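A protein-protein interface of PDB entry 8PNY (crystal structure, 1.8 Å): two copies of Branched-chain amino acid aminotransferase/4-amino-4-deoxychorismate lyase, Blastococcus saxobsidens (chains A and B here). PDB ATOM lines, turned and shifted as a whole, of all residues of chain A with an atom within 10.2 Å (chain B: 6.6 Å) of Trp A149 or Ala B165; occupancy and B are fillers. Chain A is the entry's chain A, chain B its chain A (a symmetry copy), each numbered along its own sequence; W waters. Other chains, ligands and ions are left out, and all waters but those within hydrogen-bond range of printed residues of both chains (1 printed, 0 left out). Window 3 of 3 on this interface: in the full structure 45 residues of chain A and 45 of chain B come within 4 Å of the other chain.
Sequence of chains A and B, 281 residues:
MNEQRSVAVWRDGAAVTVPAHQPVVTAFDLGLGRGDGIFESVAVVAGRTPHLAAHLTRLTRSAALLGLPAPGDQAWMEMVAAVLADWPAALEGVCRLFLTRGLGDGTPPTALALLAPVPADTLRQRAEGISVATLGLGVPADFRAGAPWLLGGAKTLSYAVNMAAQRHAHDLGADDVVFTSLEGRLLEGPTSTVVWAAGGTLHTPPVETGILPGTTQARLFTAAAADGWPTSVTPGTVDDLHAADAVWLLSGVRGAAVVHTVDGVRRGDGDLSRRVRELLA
NE1 of Trp A149 lies within hydrogen-bond range of O of Gly B136, at 2.9 Å. The backbone carbonyl oxygen (O) of Leu A66 lies within hydrogen-bond range of the guanidinium group (NH2) of Arg B167. NH2 of Arg A101 sits close to NH1 of Arg B167 (3.3 Å). OG of Ser A158 sits at hydrogen-bond distance from N of Ala B160, 3.0 Å away. The guanidinium group (NH1) of Arg B167 lies within salt-bridge range of the side-chain carboxylate (OD2) of Asp A36.
The side-chain hydroxyl (OG1) of Thr A156 sits close to the backbone NH (N) of Ser A158, at 3.1 Å. OD2 of Asp A36 is in salt-bridge range of NE of Arg A101 (2.7 Å). NH2 of Arg A101 is in hydrogen-bond range of O of Leu A66, at 2.7 Å.
Among the printed residues, pairs that only touch across the chains: Val A139 with Leu B137 (3.9 Å), Val A139 with Gly B138 (3.5 Å), Phe A143 with Gly B136 (3.96 Å), Phe A143 with Gly B138 (3.5 Å), Trp A149 with Leu B135 (3.9 Å), Trp A149 with Val B161 (3.5 Å), Trp A149 with Ala B164 (3.6 Å), Trp A149 with Ala B165 (3.7 Å), Trp A149 with His B168 (3.6 Å), Leu A150 with Leu B137 (3.8 Å), Leu A150 with Val B161 (3.6 Å), Leu A151 with Ala B160 (3.6 Å) and Leu A151 with Ala B164 (3.7 Å).
Of chain B, only Leu B135, Gly B136, Val B161, Ala B164, Ala B165 and His B168 come within 4 Å of Trp A149. Leu B135 touches just one residue of chain A: Trp A149 (3.9 Å). Gly B136 touches just these residues of chain A: Phe A143 (3.96 Å) and Trp A149 (2.9 Å). Of chain A, only Trp A149 (3.5 Å) and Leu A150 (3.6 Å) come within 4 Å of Val B161. Of chain A, only Trp A149 and Leu A151 come within 4 Å of Ala B164. Of the printed residues of chain A, His B168 touches Trp A149 (3.6 Å). Ala B169 touches none of the printed residues of chain A. Printed residues of chain B within 4 Å of Phe A143: Gly B136 and Gly B138. Of the printed residues of chain B, Arg A101 touches Arg B167. Of the printed residues of chain A, Leu B137 touches Val A139 and Leu A150. Printed residues of chain B within 4 Å of Val A139: Leu B137 (3.9 Å) and Gly B138 (3.5 Å). Of the printed residues of chain A, Arg B167 touches Asp A36 (3.8 Å), Leu A66 (3.4 Å) and Arg A101 (3.3 Å). Gly A146 touches none of the printed residues of chain B. Ala A147 touches none of the printed residues of chain B.
Hydrophobic or aromatic side chains of chain B that line the printed part of chain A: Leu B135, Ala B160, Val B161, Ala B164 and His B168.
No position is printed for both chains. Of the 18 pairs that touch across the chains among the printed residues, none has its exchanged pair printed and touching as well.
Water W1 lies within hydrogen-bond range of NH2 of Arg B167 (2.8 Å), O of Ala B160 (2.8 Å) and OD1 of Asp A36 (2.8 Å).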
ATOM      1  N   ASP A  36      -1.959 -18.502 -24.058  1.00  0.00           N
ATOM      2  CA  ASP A  36      -0.927 -19.083 -23.172  1.00  0.00           C
ATOM      3  C   ASP A  36      -1.567 -20.187 -22.327  1.00  0.00           C
ATOM      4  O   ASP A  36      -1.978 -19.948 -21.186  1.00  0.00           O
ATOM      5  CB  ASP A  36      -0.257 -17.996 -22.338  1.00  0.00           C
ATOM      6  CG  ASP A  36       1.066 -18.445 -21.738  1.00  0.00           C
ATOM      7  OD1 ASP A  36       1.515 -19.611 -22.023  1.00  0.00           O
ATOM      8  OD2 ASP A  36       1.586 -17.666 -20.918  1.00  0.00           O
ATOM      9  N   LEU A  65       5.982 -28.557 -21.201  1.00  0.00           N
ATOM     10  CA  LEU A  65       6.652 -27.713 -22.219  1.00  0.00           C
ATOM     11  C   LEU A  65       6.350 -26.232 -21.952  1.00  0.00           C
ATOM     12  O   LEU A  65       7.243 -25.418 -22.247  1.00  0.00           O
ATOM     13  CB  LEU A  65       6.231 -28.142 -23.626  1.00  0.00           C
ATOM     14  CG  LEU A  65       6.736 -29.527 -24.038  1.00  0.00           C
ATOM     15  CD1 LEU A  65       6.231 -29.912 -25.411  1.00  0.00           C
ATOM     16  CD2 LEU A  65       8.244 -29.599 -24.019  1.00  0.00           C
ATOM     17  N   LEU A  66       5.147 -25.882 -21.475  1.00  0.00           N
ATOM     18  CA  LEU A  66       4.757 -24.453 -21.291  1.00  0.00           C
ATOM     19  C   LEU A  66       5.016 -24.038 -19.848  1.00  0.00           C
ATOM     20  O   LEU A  66       4.801 -22.869 -19.548  1.00  0.00           O
ATOM     21  CB  LEU A  66       3.301 -24.224 -21.703  1.00  0.00           C
ATOM     22  CG  LEU A  66       3.177 -23.863 -23.179  1.00  0.00           C
ATOM     23  CD1 LEU A  66       3.463 -25.061 -24.072  1.00  0.00           C
ATOM     24  CD2 LEU A  66       1.852 -23.212 -23.475  1.00  0.00           C
ATOM     25  N   ARG A 101      -2.654 -20.257 -18.281  1.00  0.00           N
ATOM     26  CA  ARG A 101      -1.764 -19.701 -17.221  1.00  0.00           C
ATOM     27  C   ARG A 101      -2.578 -18.841 -16.252  1.00  0.00           C
ATOM     28  O   ARG A 101      -2.036 -18.448 -15.225  1.00  0.00           O
ATOM     29  CB  ARG A 101      -0.585 -18.944 -17.830  1.00  0.00           C
ATOM     30  CG  ARG A 101       0.584 -18.900 -16.861  1.00  0.00           C
ATOM     31  CD  ARG A 101       1.881 -18.430 -17.448  1.00  0.00           C
ATOM     32  NE  ARG A 101       2.233 -19.106 -18.684  1.00  0.00           N
ATOM     33  CZ  ARG A 101       2.890 -20.248 -18.769  1.00  0.00           C
ATOM     34  NH1 ARG A 101       3.283 -20.889 -17.681  1.00  0.00           N
ATOM     35  NH2 ARG A 101       3.161 -20.757 -19.951  1.00  0.00           N
ATOM     36  N   VAL A 139      10.026 -23.470 -41.865  1.00  0.00           N
ATOM     37  CA  VAL A 139      11.122 -23.845 -40.931  1.00  0.00           C
ATOM     38  C   VAL A 139      11.848 -25.047 -41.505  1.00  0.00           C
ATOM     39  O   VAL A 139      11.227 -25.909 -42.116  1.00  0.00           O
ATOM     40  CB  VAL A 139      10.585 -24.092 -39.515  1.00  0.00           C
ATOM     41  CG1 VAL A 139      10.041 -22.796 -38.927  1.00  0.00           C
ATOM     42  CG2 VAL A 139       9.545 -25.202 -39.482  1.00  0.00           C
ATOM     43  N   PHE A 143      14.976 -27.775 -37.347  1.00  0.00           N
ATOM     44  CA  PHE A 143      15.151 -26.489 -36.628  1.00  0.00           C
ATOM     45  C   PHE A 143      14.527 -26.551 -35.229  1.00  0.00           C
ATOM     46  O   PHE A 143      15.184 -26.127 -34.269  1.00  0.00           O
ATOM     47  CB  PHE A 143      14.592 -25.305 -37.406  1.00  0.00           C
ATOM     48  CG  PHE A 143      15.009 -24.000 -36.787  1.00  0.00           C
ATOM     49  CD1 PHE A 143      16.212 -23.412 -37.142  1.00  0.00           C
ATOM     50  CD2 PHE A 143      14.248 -23.407 -35.785  1.00  0.00           C
ATOM     51  CE1 PHE A 143      16.627 -22.226 -36.558  1.00  0.00           C
ATOM     52  CE2 PHE A 143      14.654 -22.211 -35.208  1.00  0.00           C
ATOM     53  CZ  PHE A 143      15.841 -21.624 -35.599  1.00  0.00           C
ATOM     54  N   ARG A 144      13.303 -27.051 -35.097  1.00  0.00           N
ATOM     55  CA  ARG A 144      12.538 -26.864 -33.830  1.00  0.00           C
ATOM     56  C   ARG A 144      13.195 -27.645 -32.697  1.00  0.00           C
ATOM     57  O   ARG A 144      13.096 -27.186 -31.541  1.00  0.00           O
ATOM     58  CB  ARG A 144      11.061 -27.188 -34.030  1.00  0.00           C
ATOM     59  CG  ARG A 144      10.345 -26.028 -34.693  1.00  0.00           C
ATOM     60  CD  ARG A 144       8.886 -26.267 -34.950  1.00  0.00           C
ATOM     61  NE  ARG A 144       8.700 -27.374 -35.847  1.00  0.00           N
ATOM     62  CZ  ARG A 144       7.526 -27.732 -36.358  1.00  0.00           C
ATOM     63  NH1 ARG A 144       6.446 -27.023 -36.094  1.00  0.00           N
ATOM     64  NH2 ARG A 144       7.441 -28.817 -37.102  1.00  0.00           N
ATOM     65  N   ALA A 145      13.904 -28.725 -33.015  1.00  0.00           N
ATOM     66  CA  ALA A 145      14.650 -29.539 -32.038  1.00  0.00           C
ATOM     67  C   ALA A 145      15.616 -28.647 -31.246  1.00  0.00           C
ATOM     68  O   ALA A 145      15.778 -28.897 -30.030  1.00  0.00           O
ATOM     69  CB  ALA A 145      15.375 -30.660 -32.761  1.00  0.00           C
ATOM     70  N   GLY A 146      16.200 -27.629 -31.885  1.00  0.00           N
ATOM     71  CA  GLY A 146      17.129 -26.688 -31.232  1.00  0.00           C
ATOM     72  C   GLY A 146      16.468 -25.400 -30.739  1.00  0.00           C
ATOM     73  O   GLY A 146      17.219 -24.479 -30.372  1.00  0.00           O
ATOM     74  N   ALA A 147      15.136 -25.289 -30.793  1.00  0.00           N
ATOM     75  CA  ALA A 147      14.390 -24.020 -30.570  1.00  0.00           C
ATOM     76  C   ALA A 147      13.141 -24.308 -29.742  1.00  0.00           C
ATOM     77  O   ALA A 147      12.026 -24.260 -30.260  1.00  0.00           O
ATOM     78  CB  ALA A 147      14.061 -23.381 -31.903  1.00  0.00           C
ATOM     79  N   PRO A 148      13.311 -24.691 -28.457  1.00  0.00           N
ATOM     80  CA  PRO A 148      12.191 -25.077 -27.602  1.00  0.00           C
ATOM     81  C   PRO A 148      11.124 -23.975 -27.478  1.00  0.00           C
ATOM     82  O   PRO A 148       9.992 -24.309 -27.292  1.00  0.00           O
ATOM     83  CB  PRO A 148      12.878 -25.357 -26.253  1.00  0.00           C
ATOM     84  CG  PRO A 148      14.177 -24.577 -26.318  1.00  0.00           C
ATOM     85  CD  PRO A 148      14.600 -24.817 -27.745  1.00  0.00           C
ATOM     86  N   TRP A 149      11.514 -22.698 -27.573  1.00  0.00           N
ATOM     87  CA  TRP A 149      10.566 -21.547 -27.516  1.00  0.00           C
ATOM     88  C   TRP A 149       9.516 -21.628 -28.638  1.00  0.00           C
ATOM     89  O   TRP A 149       8.514 -20.948 -28.508  1.00  0.00           O
ATOM     90  CB  TRP A 149      11.326 -20.215 -27.542  1.00  0.00           C
ATOM     91  CG  TRP A 149      12.256 -20.041 -28.700  1.00  0.00           C
ATOM     92  CD1 TRP A 149      11.973 -19.497 -29.908  1.00  0.00           C
ATOM     93  CD2 TRP A 149      13.644 -20.422 -28.749  1.00  0.00           C
ATOM     94  NE1 TRP A 149      13.091 -19.485 -30.697  1.00  0.00           N
ATOM     95  CE2 TRP A 149      14.112 -20.109 -30.036  1.00  0.00           C
ATOM     96  CE3 TRP A 149      14.519 -21.028 -27.844  1.00  0.00           C
ATOM     97  CZ2 TRP A 149      15.424 -20.342 -30.435  1.00  0.00           C
ATOM     98  CZ3 TRP A 149      15.813 -21.266 -28.237  1.00  0.00           C
ATOM     99  CH2 TRP A 149      16.263 -20.916 -29.508  1.00  0.00           C
ATOM    100  N   LEU A 150       9.749 -22.364 -29.741  1.00  0.00           N
ATOM    101  CA  LEU A 150       8.724 -22.541 -30.816  1.00  0.00           C
ATOM    102  C   LEU A 150       7.634 -23.552 -30.409  1.00  0.00           C
ATOM    103  O   LEU A 150       6.648 -23.668 -31.157  1.00  0.00           O
ATOM    104  CB  LEU A 150       9.413 -22.961 -32.113  1.00  0.00           C
ATOM    105  CG  LEU A 150      10.382 -21.928 -32.685  1.00  0.00           C
ATOM    106  CD1 LEU A 150      11.008 -22.437 -33.980  1.00  0.00           C
ATOM    107  CD2 LEU A 150       9.684 -20.599 -32.909  1.00  0.00           C
ATOM    108  N   LEU A 151       7.764 -24.224 -29.262  1.00  0.00           N
ATOM    109  CA  LEU A 151       6.698 -25.079 -28.664  1.00  0.00           C
ATOM    110  C   LEU A 151       6.252 -26.212 -29.620  1.00  0.00           C
ATOM    111  O   LEU A 151       5.067 -26.630 -29.524  1.00  0.00           O
ATOM    112  CB  LEU A 151       5.524 -24.192 -28.256  1.00  0.00           C
ATOM    113  CG  LEU A 151       5.867 -23.080 -27.253  1.00  0.00           C
ATOM    114  CD1 LEU A 151       4.623 -22.329 -26.796  1.00  0.00           C
ATOM    115  CD2 LEU A 151       6.593 -23.653 -26.052  1.00  0.00           C
ATOM    116  N   GLY A 152       7.170 -26.723 -30.446  1.00  0.00           N
ATOM    117  CA  GLY A 152       6.935 -27.750 -31.485  1.00  0.00           C
ATOM    118  C   GLY A 152       6.139 -28.964 -31.002  1.00  0.00           C
ATOM    119  O   GLY A 152       5.166 -29.369 -31.719  1.00  0.00           O
ATOM    120  N   GLY A 153       6.495 -29.553 -29.856  1.00  0.00           N
ATOM    121  CA  GLY A 153       5.807 -30.774 -29.373  1.00  0.00           C
ATOM    122  C   GLY A 153       4.657 -30.495 -28.399  1.00  0.00           C
ATOM    123  O   GLY A 153       4.238 -31.438 -27.698  1.00  0.00           O
ATOM    124  N   ALA A 154       4.152 -29.256 -28.327  1.00  0.00           N
ATOM    125  CA  ALA A 154       3.087 -28.836 -27.385  1.00  0.00           C
ATOM    126  C   ALA A 154       1.808 -28.539 -28.166  1.00  0.00           C
ATOM    127  O   ALA A 154       1.904 -28.012 -29.272  1.00  0.00           O
ATOM    128  CB  ALA A 154       3.540 -27.629 -26.601  1.00  0.00           C
ATOM    129  N   THR A 156      -1.243 -26.155 -28.021  1.00  0.00           N
ATOM    130  CA  THR A 156      -1.484 -24.881 -27.294  1.00  0.00           C
ATOM    131  C   THR A 156      -2.823 -24.284 -27.691  1.00  0.00           C
ATOM    132  O   THR A 156      -3.388 -24.695 -28.699  1.00  0.00           O
ATOM    133  CB  THR A 156      -0.360 -23.866 -27.517  1.00  0.00           C
ATOM    134  OG1 THR A 156      -0.454 -23.349 -28.839  1.00  0.00           O
ATOM    135  CG2 THR A 156       1.023 -24.434 -27.301  1.00  0.00           C
ATOM    136  N   SER A 158      -2.916 -21.441 -28.841  1.00  0.00           N
ATOM    137  CA  SER A 158      -2.418 -20.448 -29.821  1.00  0.00           C
ATOM    138  C   SER A 158      -2.463 -21.022 -31.225  1.00  0.00           C
ATOM    139  O   SER A 158      -1.389 -21.386 -31.734  1.00  0.00           O
ATOM    140  CB  SER A 158      -1.025 -20.068 -29.509  1.00  0.00           C
ATOM    141  OG  SER A 158      -1.014 -18.970 -28.659  1.00  0.00           O
ATOM    142  N   GLY A 210       9.859 -31.690 -34.534  1.00  0.00           N
ATOM    143  CA  GLY A 210       9.136 -30.797 -33.614  1.00  0.00           C
ATOM    144  C   GLY A 210       7.645 -30.772 -33.889  1.00  0.00           C
ATOM    145  O   GLY A 210       7.055 -29.690 -33.782  1.00  0.00           O
ATOM    146  N   ALA B 133      17.938 -10.998 -25.654  1.00  0.00           N
ATOM    147  CA  ALA B 133      18.404 -12.268 -26.240  1.00  0.00           C
ATOM    148  C   ALA B 133      17.935 -12.281 -27.694  1.00  0.00           C
ATOM    149  O   ALA B 133      16.754 -11.968 -27.932  1.00  0.00           O
ATOM    150  CB  ALA B 133      17.807 -13.434 -25.491  1.00  0.00           C
ATOM    151  N   THR B 134      18.789 -12.658 -28.619  1.00  0.00           N
ATOM    152  CA  THR B 134      18.363 -12.938 -30.012  1.00  0.00           C
ATOM    153  C   THR B 134      17.986 -14.415 -30.103  1.00  0.00           C
ATOM    154  O   THR B 134      18.757 -15.259 -29.622  1.00  0.00           O
ATOM    155  CB  THR B 134      19.410 -12.492 -31.040  1.00  0.00           C
ATOM    156  OG1 THR B 134      20.593 -13.277 -30.892  1.00  0.00           O
ATOM    157  CG2 THR B 134      19.715 -11.020 -30.925  1.00  0.00           C
ATOM    158  N   LEU B 135      16.815 -14.717 -30.651  1.00  0.00           N
ATOM    159  CA  LEU B 135      16.329 -16.096 -30.796  1.00  0.00           C
ATOM    160  C   LEU B 135      15.856 -16.272 -32.240  1.00  0.00           C
ATOM    161  O   LEU B 135      15.171 -15.375 -32.745  1.00  0.00           O
ATOM    162  CB  LEU B 135      15.206 -16.348 -29.783  1.00  0.00           C
ATOM    163  CG  LEU B 135      15.592 -16.265 -28.302  1.00  0.00           C
ATOM    164  CD1 LEU B 135      14.371 -16.458 -27.406  1.00  0.00           C
ATOM    165  CD2 LEU B 135      16.650 -17.300 -27.914  1.00  0.00           C
ATOM    166  N   GLY B 136      16.255 -17.364 -32.888  1.00  0.00           N
ATOM    167  CA  GLY B 136      15.808 -17.612 -34.269  1.00  0.00           C
ATOM    168  C   GLY B 136      14.359 -18.055 -34.291  1.00  0.00           C
ATOM    169  O   GLY B 136      13.931 -18.770 -33.381  1.00  0.00           O
ATOM    170  N   LEU B 137      13.620 -17.611 -35.292  1.00  0.00           N
ATOM    171  CA  LEU B 137      12.233 -18.024 -35.584  1.00  0.00           C
ATOM    172  C   LEU B 137      12.250 -19.200 -36.556  1.00  0.00           C
ATOM    173  O   LEU B 137      11.207 -19.826 -36.712  1.00  0.00           O
ATOM    174  CB  LEU B 137      11.536 -16.808 -36.171  1.00  0.00           C
ATOM    175  CG  LEU B 137      10.173 -16.479 -35.597  1.00  0.00           C
ATOM    176  CD1 LEU B 137      10.174 -16.590 -34.080  1.00  0.00           C
ATOM    177  CD2 LEU B 137       9.741 -15.095 -36.059  1.00  0.00           C
ATOM    178  N   GLY B 138      13.392 -19.486 -37.183  1.00  0.00           N
ATOM    179  CA  GLY B 138      13.541 -20.593 -38.138  1.00  0.00           C
ATOM    180  C   GLY B 138      13.101 -20.252 -39.548  1.00  0.00           C
ATOM    181  O   GLY B 138      13.272 -21.073 -40.429  1.00  0.00           O
ATOM    182  N   ALA B 160       1.491 -17.715 -27.732  1.00  0.00           N
ATOM    183  CA  ALA B 160       2.119 -18.736 -26.869  1.00  0.00           C
ATOM    184  C   ALA B 160       3.619 -18.756 -27.162  1.00  0.00           C
ATOM    185  O   ALA B 160       4.436 -18.788 -26.225  1.00  0.00           O
ATOM    186  CB  ALA B 160       1.481 -20.097 -27.056  1.00  0.00           C
ATOM    187  N   VAL B 161       3.998 -18.697 -28.426  1.00  0.00           N
ATOM    188  CA  VAL B 161       5.439 -18.749 -28.788  1.00  0.00           C
ATOM    189  C   VAL B 161       6.142 -17.494 -28.266  1.00  0.00           C
ATOM    190  O   VAL B 161       7.276 -17.629 -27.744  1.00  0.00           O
ATOM    191  CB  VAL B 161       5.644 -18.945 -30.300  1.00  0.00           C
ATOM    192  CG1 VAL B 161       7.077 -18.706 -30.728  1.00  0.00           C
ATOM    193  CG2 VAL B 161       5.218 -20.359 -30.674  1.00  0.00           C
ATOM    194  N   ASN B 162       5.516 -16.342 -28.493  1.00  0.00           N
ATOM    195  CA  ASN B 162       5.983 -14.995 -28.078  1.00  0.00           C
ATOM    196  C   ASN B 162       6.311 -15.047 -26.579  1.00  0.00           C
ATOM    197  O   ASN B 162       7.356 -14.655 -26.195  1.00  0.00           O
ATOM    198  CB  ASN B 162       4.908 -13.961 -28.428  1.00  0.00           C
ATOM    199  CG  ASN B 162       4.369 -14.109 -29.843  1.00  0.00           C
ATOM    200  OD1 ASN B 162       3.799 -15.148 -30.235  1.00  0.00           O
ATOM    201  ND2 ASN B 162       4.583 -13.079 -30.627  1.00  0.00           N
ATOM    202  N   MET B 163       5.376 -15.554 -25.791  1.00  0.00           N
ATOM    203  CA  MET B 163       5.539 -15.695 -24.325  1.00  0.00           C
ATOM    204  C   MET B 163       6.633 -16.715 -23.977  1.00  0.00           C
ATOM    205  O   MET B 163       7.418 -16.431 -23.041  1.00  0.00           O
ATOM    206  CB  MET B 163       4.217 -16.069 -23.655  1.00  0.00           C
ATOM    207  CG  MET B 163       3.153 -15.010 -23.859  1.00  0.00           C
ATOM    208  SD  MET B 163       3.587 -13.297 -23.402  1.00  0.00           S
ATOM    209  CE  MET B 163       4.156 -12.572 -24.932  1.00  0.00           C
ATOM    210  N   ALA B 164       6.707 -17.854 -24.663  1.00  0.00           N
ATOM    211  CA  ALA B 164       7.731 -18.893 -24.386  1.00  0.00           C
ATOM    212  C   ALA B 164       9.120 -18.350 -24.747  1.00  0.00           C
ATOM    213  O   ALA B 164      10.084 -18.647 -24.013  1.00  0.00           O
ATOM    214  CB  ALA B 164       7.457 -20.141 -25.158  1.00  0.00           C
ATOM    215  N   ALA B 165       9.218 -17.541 -25.794  1.00  0.00           N
ATOM    216  CA  ALA B 165      10.484 -16.878 -26.174  1.00  0.00           C
ATOM    217  C   ALA B 165      10.937 -15.986 -25.027  1.00  0.00           C
ATOM    218  O   ALA B 165      12.143 -16.027 -24.628  1.00  0.00           O
ATOM    219  CB  ALA B 165      10.305 -16.114 -27.450  1.00  0.00           C
ATOM    220  N   GLN B 166      10.018 -15.217 -24.493  1.00  0.00           N
ATOM    221  CA  GLN B 166      10.340 -14.292 -23.370  1.00  0.00           C
ATOM    222  C   GLN B 166      10.759 -15.097 -22.133  1.00  0.00           C
ATOM    223  O   GLN B 166      11.707 -14.680 -21.424  1.00  0.00           O
ATOM    224  CB  GLN B 166       9.184 -13.344 -23.121  1.00  0.00           C
ATOM    225  CG  GLN B 166       9.019 -12.394 -24.311  1.00  0.00           C
ATOM    226  CD  GLN B 166       8.104 -11.240 -24.014  1.00  0.00           C
ATOM    227  OE1 GLN B 166       7.027 -11.415 -23.434  1.00  0.00           O
ATOM    228  NE2 GLN B 166       8.531 -10.056 -24.435  1.00  0.00           N
ATOM    229  N   ARG B 167      10.083 -16.197 -21.841  1.00  0.00           N
ATOM    230  CA  ARG B 167      10.467 -17.024 -20.668  1.00  0.00           C
ATOM    231  C   ARG B 167      11.858 -17.597 -20.898  1.00  0.00           C
ATOM    232  O   ARG B 167      12.710 -17.586 -19.920  1.00  0.00           O
ATOM    233  CB  ARG B 167       9.437 -18.125 -20.398  1.00  0.00           C
ATOM    234  CG  ARG B 167       8.142 -17.573 -19.819  1.00  0.00           C
ATOM    235  CD  ARG B 167       7.201 -18.622 -19.246  1.00  0.00           C
ATOM    236  NE  ARG B 167       6.957 -19.725 -20.181  1.00  0.00           N
ATOM    237  CZ  ARG B 167       6.009 -19.695 -21.129  1.00  0.00           C
ATOM    238  NH1 ARG B 167       5.276 -18.606 -21.269  1.00  0.00           N
ATOM    239  NH2 ARG B 167       5.851 -20.732 -21.934  1.00  0.00           N
ATOM    240  N   HIS B 168      12.130 -18.059 -22.111  1.00  0.00           N
ATOM    241  CA  HIS B 168      13.441 -18.639 -22.464  1.00  0.00           C
ATOM    242  C   HIS B 168      14.527 -17.591 -22.212  1.00  0.00           C
ATOM    243  O   HIS B 168      15.563 -17.937 -21.604  1.00  0.00           O
ATOM    244  CB  HIS B 168      13.472 -19.090 -23.907  1.00  0.00           C
ATOM    245  CG  HIS B 168      14.792 -19.662 -24.272  1.00  0.00           C
ATOM    246  ND1 HIS B 168      15.059 -20.988 -24.105  1.00  0.00           N
ATOM    247  CD2 HIS B 168      15.886 -19.109 -24.831  1.00  0.00           C
ATOM    248  CE1 HIS B 168      16.273 -21.245 -24.551  1.00  0.00           C
ATOM    249  NE2 HIS B 168      16.813 -20.112 -24.996  1.00  0.00           N
ATOM    250  N   ALA B 169      14.296 -16.374 -22.684  1.00  0.00           N
ATOM    251  CA  ALA B 169      15.176 -15.196 -22.455  1.00  0.00           C
ATOM    252  C   ALA B 169      15.360 -14.900 -20.948  1.00  0.00           C
ATOM    253  O   ALA B 169      16.536 -14.745 -20.545  1.00  0.00           O
ATOM    254  CB  ALA B 169      14.615 -14.021 -23.200  1.00  0.00           C
ATOM    255  N   HIS B 170      14.282 -14.856 -20.147  1.00  0.00           N
ATOM    256  CA  HIS B 170      14.355 -14.621 -18.680  1.00  0.00           C
ATOM    257  C   HIS B 170      15.264 -15.698 -18.066  1.00  0.00           C
ATOM    258  O   HIS B 170      16.133 -15.340 -17.245  1.00  0.00           O
ATOM    259  CB  HIS B 170      12.945 -14.557 -18.073  1.00  0.00           C
ATOM    260  CG  HIS B 170      12.015 -13.561 -18.706  1.00  0.00           C
ATOM    261  ND1 HIS B 170      10.638 -13.755 -18.774  1.00  0.00           N
ATOM    262  CD2 HIS B 170      12.253 -12.398 -19.351  1.00  0.00           C
ATOM    263  CE1 HIS B 170      10.077 -12.738 -19.390  1.00  0.00           C
ATOM    264  NE2 HIS B 170      11.037 -11.883 -19.734  1.00  0.00           N
ATOM    265  N   ASP B 176      14.278  -9.397 -22.598  1.00  0.00           N
ATOM    266  CA  ASP B 176      13.422  -9.377 -23.816  1.00  0.00           C
ATOM    267  C   ASP B 176      14.161 -10.019 -24.985  1.00  0.00           C
ATOM    268  O   ASP B 176      15.277 -10.513 -24.834  1.00  0.00           O
ATOM    269  CB  ASP B 176      12.961  -7.953 -24.129  1.00  0.00           C
ATOM    270  CG  ASP B 176      11.551  -7.859 -24.698  1.00  0.00           C
ATOM    271  OD1 ASP B 176      11.076  -8.871 -25.310  1.00  0.00           O
ATOM    272  OD2 ASP B 176      10.928  -6.808 -24.490  1.00  0.00           O
ATOM    273  N   VAL B 177      13.483 -10.055 -26.110  1.00  0.00           N
ATOM    274  CA  VAL B 177      13.866 -10.913 -27.250  1.00  0.00           C
ATOM    275  C   VAL B 177      13.855 -10.058 -28.505  1.00  0.00           C
ATOM    276  O   VAL B 177      12.926  -9.246 -28.710  1.00  0.00           O
ATOM    277  CB  VAL B 177      12.879 -12.073 -27.379  1.00  0.00           C
ATOM    278  CG1 VAL B 177      13.063 -12.715 -28.740  1.00  0.00           C
ATOM    279  CG2 VAL B 177      13.063 -13.065 -26.240  1.00  0.00           C
ATOM    280  N   PHE B 179      13.749 -11.449 -32.430  1.00  0.00           N
ATOM    281  CA  PHE B 179      13.746 -12.632 -33.327  1.00  0.00           C
ATOM    282  C   PHE B 179      14.668 -12.384 -34.519  1.00  0.00           C
ATOM    283  O   PHE B 179      14.747 -11.234 -35.043  1.00  0.00           O
ATOM    284  CB  PHE B 179      12.341 -12.998 -33.806  1.00  0.00           C
ATOM    285  CG  PHE B 179      11.448 -13.586 -32.744  1.00  0.00           C
ATOM    286  CD1 PHE B 179      11.888 -14.641 -31.972  1.00  0.00           C
ATOM    287  CD2 PHE B 179      10.178 -13.075 -32.506  1.00  0.00           C
ATOM    288  CE1 PHE B 179      11.061 -15.226 -31.024  1.00  0.00           C
ATOM    289  CE2 PHE B 179       9.363 -13.628 -31.529  1.00  0.00           C
ATOM    290  CZ  PHE B 179       9.811 -14.689 -30.780  1.00  0.00           C
ATOM    291  N   PRO B 190       8.956 -10.249 -29.902  1.00  0.00           N
ATOM    292  CA  PRO B 190       7.628 -10.736 -29.536  1.00  0.00           C
ATOM    293  C   PRO B 190       6.649  -9.568 -29.325  1.00  0.00           C
ATOM    294  O   PRO B 190       5.514  -9.695 -29.725  1.00  0.00           O
ATOM    295  CB  PRO B 190       7.911 -11.503 -28.236  1.00  0.00           C
ATOM    296  CG  PRO B 190       9.334 -12.022 -28.399  1.00  0.00           C
ATOM    297  CD  PRO B 190      10.047 -11.040 -29.309  1.00  0.00           C
HETATM  298  O   HOH W   1       3.828 -19.800 -23.654  1.00  0.00           O
